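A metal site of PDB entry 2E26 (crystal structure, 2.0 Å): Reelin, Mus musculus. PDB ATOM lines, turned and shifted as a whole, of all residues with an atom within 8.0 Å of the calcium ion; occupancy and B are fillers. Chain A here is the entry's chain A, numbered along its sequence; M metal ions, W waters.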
ATOM      1  N   ASP A 227      12.909 -34.383  12.614  1.00  0.00           N
ATOM      2  CA  ASP A 227      13.422 -33.052  12.944  1.00  0.00           C
ATOM      3  C   ASP A 227      13.209 -32.687  14.403  1.00  0.00           C
ATOM      4  O   ASP A 227      12.070 -32.633  14.880  1.00  0.00           O
ATOM      5  CB  ASP A 227      12.867 -31.961  12.016  1.00  0.00           C
ATOM      6  CG  ASP A 227      13.889 -30.858  11.748  1.00  0.00           C
ATOM      7  OD1 ASP A 227      14.024 -30.419  10.576  1.00  0.00           O
ATOM      8  OD2 ASP A 227      14.578 -30.441  12.698  1.00  0.00           O
ATOM      9  N   ASP A 228      14.318 -32.450  15.100  1.00  0.00           N
ATOM     10  CA  ASP A 228      14.295 -31.995  16.481  1.00  0.00           C
ATOM     11  C   ASP A 228      14.492 -30.473  16.573  1.00  0.00           C
ATOM     12  O   ASP A 228      14.483 -29.883  17.658  1.00  0.00           O
ATOM     13  CB  ASP A 228      15.386 -32.712  17.286  1.00  0.00           C
ATOM     14  CG  ASP A 228      16.779 -32.495  16.711  1.00  0.00           C
ATOM     15  OD1 ASP A 228      16.984 -31.675  15.787  1.00  0.00           O
ATOM     16  OD2 ASP A 228      17.709 -33.165  17.213  1.00  0.00           O
ATOM     17  N   PHE A 229      14.686 -29.857  15.402  1.00  0.00           N
ATOM     18  CA  PHE A 229      14.885 -28.409  15.267  1.00  0.00           C
ATOM     19  C   PHE A 229      16.144 -27.868  15.940  1.00  0.00           C
ATOM     20  O   PHE A 229      16.248 -26.674  16.187  1.00  0.00           O
ATOM     21  CB  PHE A 229      13.607 -27.636  15.685  1.00  0.00           C
ATOM     22  CG  PHE A 229      12.396 -28.058  14.913  1.00  0.00           C
ATOM     23  CD1 PHE A 229      12.282 -27.748  13.564  1.00  0.00           C
ATOM     24  CD2 PHE A 229      11.394 -28.804  15.521  1.00  0.00           C
ATOM     25  CE1 PHE A 229      11.183 -28.159  12.841  1.00  0.00           C
ATOM     26  CE2 PHE A 229      10.280 -29.231  14.800  1.00  0.00           C
ATOM     27  CZ  PHE A 229      10.182 -28.905  13.449  1.00  0.00           C
ATOM     28  N   GLU A 230      17.093 -28.755  16.219  1.00  0.00           N
ATOM     29  CA  GLU A 230      18.402 -28.376  16.756  1.00  0.00           C
ATOM     30  C   GLU A 230      19.423 -28.202  15.634  1.00  0.00           C
ATOM     31  O   GLU A 230      20.530 -27.716  15.877  1.00  0.00           O
ATOM     32  CB  GLU A 230      18.956 -29.439  17.725  1.00  0.00           C
ATOM     33  CG  GLU A 230      17.974 -30.162  18.636  1.00  0.00           C
ATOM     34  CD  GLU A 230      17.271 -29.271  19.613  1.00  0.00           C
ATOM     35  OE1 GLU A 230      17.624 -28.078  19.707  1.00  0.00           O
ATOM     36  OE2 GLU A 230      16.341 -29.769  20.303  1.00  0.00           O
ATOM     37  N   GLY A 231      19.055 -28.609  14.425  1.00  0.00           N
ATOM     38  CA  GLY A 231      19.983 -28.612  13.297  1.00  0.00           C
ATOM     39  C   GLY A 231      19.738 -27.452  12.369  1.00  0.00           C
ATOM     40  O   GLY A 231      19.664 -26.290  12.804  1.00  0.00           O
ATOM     41  N   SER A 247      13.125 -21.700  18.449  1.00  0.00           N
ATOM     42  CA  SER A 247      12.967 -20.916  19.660  1.00  0.00           C
ATOM     43  C   SER A 247      13.073 -21.759  20.919  1.00  0.00           C
ATOM     44  O   SER A 247      12.855 -22.966  20.889  1.00  0.00           O
ATOM     45  CB  SER A 247      11.613 -20.204  19.643  1.00  0.00           C
ATOM     46  OG  SER A 247      11.530 -19.255  20.699  1.00  0.00           O
ATOM     47  N   LEU A 253      10.159 -29.482  25.813  1.00  0.00           N
ATOM     48  CA  LEU A 253      11.294 -30.253  26.312  1.00  0.00           C
ATOM     49  C   LEU A 253      12.235 -29.363  27.117  1.00  0.00           C
ATOM     50  O   LEU A 253      12.291 -28.145  26.895  1.00  0.00           O
ATOM     51  CB  LEU A 253      12.030 -30.939  25.149  1.00  0.00           C
ATOM     52  CG  LEU A 253      11.166 -31.747  24.166  1.00  0.00           C
ATOM     53  CD1 LEU A 253      12.064 -32.435  23.163  1.00  0.00           C
ATOM     54  CD2 LEU A 253      10.266 -32.764  24.870  1.00  0.00           C
ATOM     55  N   SER A 255      15.561 -29.262  27.208  1.00  0.00           N
ATOM     56  CA  SER A 255      16.676 -28.728  26.430  1.00  0.00           C
ATOM     57  C   SER A 255      16.374 -28.677  24.931  1.00  0.00           C
ATOM     58  O   SER A 255      15.569 -29.453  24.406  1.00  0.00           O
ATOM     59  CB  SER A 255      17.972 -29.502  26.702  1.00  0.00           C
ATOM     60  OG  SER A 255      17.941 -30.728  26.001  1.00  0.00           O
ATOM     61  N   GLY A 256      17.028 -27.733  24.265  1.00  0.00           N
ATOM     62  CA  GLY A 256      16.904 -27.598  22.833  1.00  0.00           C
ATOM     63  C   GLY A 256      15.783 -26.716  22.323  1.00  0.00           C
ATOM     64  O   GLY A 256      14.816 -26.395  23.046  1.00  0.00           O
ATOM     65  N   ASN A 257      15.927 -26.319  21.066  1.00  0.00           N
ATOM     66  CA  ASN A 257      14.963 -25.498  20.380  1.00  0.00           C
ATOM     67  C   ASN A 257      13.744 -26.300  19.949  1.00  0.00           C
ATOM     68  O   ASN A 257      13.827 -27.511  19.746  1.00  0.00           O
ATOM     69  CB  ASN A 257      15.631 -24.850  19.165  1.00  0.00           C
ATOM     70  CG  ASN A 257      16.679 -23.835  19.532  1.00  0.00           C
ATOM     71  OD1 ASN A 257      16.451 -22.981  20.401  1.00  0.00           O
ATOM     72  ND2 ASN A 257      17.835 -23.911  18.887  1.00  0.00           N
ATOM     73  N   ASN A 258      12.621 -25.608  19.814  1.00  0.00           N
ATOM     74  CA  ASN A 258      11.407 -26.150  19.203  1.00  0.00           C
ATOM     75  C   ASN A 258      11.120 -25.345  17.940  1.00  0.00           C
ATOM     76  O   ASN A 258      11.833 -24.383  17.660  1.00  0.00           O
ATOM     77  CB  ASN A 258      10.255 -26.040  20.205  1.00  0.00           C
ATOM     78  CG  ASN A 258       9.988 -24.593  20.645  1.00  0.00           C
ATOM     79  OD1 ASN A 258       9.653 -23.735  19.831  1.00  0.00           O
ATOM     80  ND2 ASN A 258      10.100 -24.330  21.944  1.00  0.00           N
ATOM     81  N   LEU A 259      10.095 -25.708  17.182  1.00  0.00           N
ATOM     82  CA  LEU A 259       9.602 -24.817  16.116  1.00  0.00           C
ATOM     83  C   LEU A 259       8.382 -24.042  16.614  1.00  0.00           C
ATOM     84  O   LEU A 259       7.380 -24.614  17.031  1.00  0.00           O
ATOM     85  CB  LEU A 259       9.268 -25.585  14.832  1.00  0.00           C
ATOM     86  CG  LEU A 259       9.051 -24.736  13.565  1.00  0.00           C
ATOM     87  CD1 LEU A 259      10.356 -24.081  13.088  1.00  0.00           C
ATOM     88  CD2 LEU A 259       8.497 -25.643  12.456  1.00  0.00           C
ATOM     89  N   PHE A 285       5.851 -33.572  19.660  1.00  0.00           N
ATOM     90  CA  PHE A 285       5.363 -32.904  20.854  1.00  0.00           C
ATOM     91  C   PHE A 285       4.720 -31.616  20.366  1.00  0.00           C
ATOM     92  O   PHE A 285       5.192 -31.010  19.394  1.00  0.00           O
ATOM     93  CB  PHE A 285       6.501 -32.587  21.833  1.00  0.00           C
ATOM     94  CG  PHE A 285       7.138 -33.805  22.465  1.00  0.00           C
ATOM     95  CD1 PHE A 285       6.793 -34.186  23.763  1.00  0.00           C
ATOM     96  CD2 PHE A 285       8.094 -34.554  21.766  1.00  0.00           C
ATOM     97  CE1 PHE A 285       7.401 -35.306  24.363  1.00  0.00           C
ATOM     98  CE2 PHE A 285       8.695 -35.695  22.347  1.00  0.00           C
ATOM     99  CZ  PHE A 285       8.347 -36.067  23.645  1.00  0.00           C
ATOM    100  N   ILE A 364       5.754 -26.852  18.043  1.00  0.00           N
ATOM    101  CA  ILE A 364       5.905 -28.264  17.730  1.00  0.00           C
ATOM    102  C   ILE A 364       7.393 -28.637  17.869  1.00  0.00           C
ATOM    103  O   ILE A 364       8.282 -27.808  17.602  1.00  0.00           O
ATOM    104  CB  ILE A 364       5.345 -28.609  16.307  1.00  0.00           C
ATOM    105  CG1 ILE A 364       5.280 -30.119  16.086  1.00  0.00           C
ATOM    106  CG2 ILE A 364       6.151 -27.894  15.197  1.00  0.00           C
ATOM    107  CD1 ILE A 364       4.488 -30.534  14.841  1.00  0.00           C
ATOM    108  N   ASP A 365       7.651 -29.866  18.303  1.00  0.00           N
ATOM    109  CA  ASP A 365       9.018 -30.316  18.517  1.00  0.00           C
ATOM    110  C   ASP A 365       9.175 -31.805  18.262  1.00  0.00           C
ATOM    111  O   ASP A 365       8.189 -32.554  18.346  1.00  0.00           O
ATOM    112  CB  ASP A 365       9.471 -29.997  19.951  1.00  0.00           C
ATOM    113  CG  ASP A 365      10.974 -29.825  20.077  1.00  0.00           C
ATOM    114  OD1 ASP A 365      11.681 -29.918  19.034  1.00  0.00           O
ATOM    115  OD2 ASP A 365      11.465 -29.573  21.207  1.00  0.00           O
ATOM    116  N   GLN A 366      10.404 -32.236  17.973  1.00  0.00           N
ATOM    117  CA  GLN A 366      10.757 -33.668  17.935  1.00  0.00           C
ATOM    118  C   GLN A 366       9.865 -34.481  17.019  1.00  0.00           C
ATOM    119  O   GLN A 366       9.272 -35.490  17.446  1.00  0.00           O
ATOM    120  CB  GLN A 366      10.715 -34.318  19.329  1.00  0.00           C
ATOM    121  CG  GLN A 366      11.668 -33.779  20.350  1.00  0.00           C
ATOM    122  CD  GLN A 366      13.058 -33.589  19.826  1.00  0.00           C
ATOM    123  OE1 GLN A 366      13.602 -32.482  19.920  1.00  0.00           O
ATOM    124  NE2 GLN A 366      13.642 -34.658  19.247  1.00  0.00           N
ATOM    125  N   ILE A 367       9.750 -34.043  15.775  1.00  0.00           N
ATOM    126  CA  ILE A 367       8.919 -34.725  14.797  1.00  0.00           C
ATOM    127  C   ILE A 367       9.660 -35.951  14.307  1.00  0.00           C
ATOM    128  O   ILE A 367      10.838 -35.873  13.925  1.00  0.00           O
ATOM    129  CB  ILE A 367       8.575 -33.815  13.589  1.00  0.00           C
ATOM    130  CG1 ILE A 367       7.760 -32.602  14.064  1.00  0.00           C
ATOM    131  CG2 ILE A 367       7.820 -34.622  12.502  1.00  0.00           C
ATOM    132  CD1 ILE A 367       7.497 -31.527  12.954  1.00  0.00           C
HETATM  133 CA    CA M   1      13.933 -29.706  19.917  1.00  0.00          CA
HETATM  134  O   HOH W   1      13.981 -29.690  22.265  1.00  0.00           O
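The backbone NH of Phe 285 sits at hydrogen-bond distance from the backbone carbonyl oxygen of Asp 365, 2.9 Å away.
O of Asn 257 binds the calcium ion, at 2.2 Å. O of Asp 228 binds the calcium ion (2.3 Å). The calcium ion is bound by water W1. OD1 of Asp 365 binds the calcium ion, at 2.4 Å. The calcium ion is bound by the side-chain carboxylate (OE2) of Glu 230, 2.4 Å away. OD2 of Asp 365 binds the calcium ion, at 2.8 Å. The side-chain amide oxygen (OE1) of Gln 366 binds the calcium ion (2.8 Å).
Five residues have an atom within 4 Å of the calcium ion: Asp 228, Glu 230, Asn 257, Asp 365 and Gln 366.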
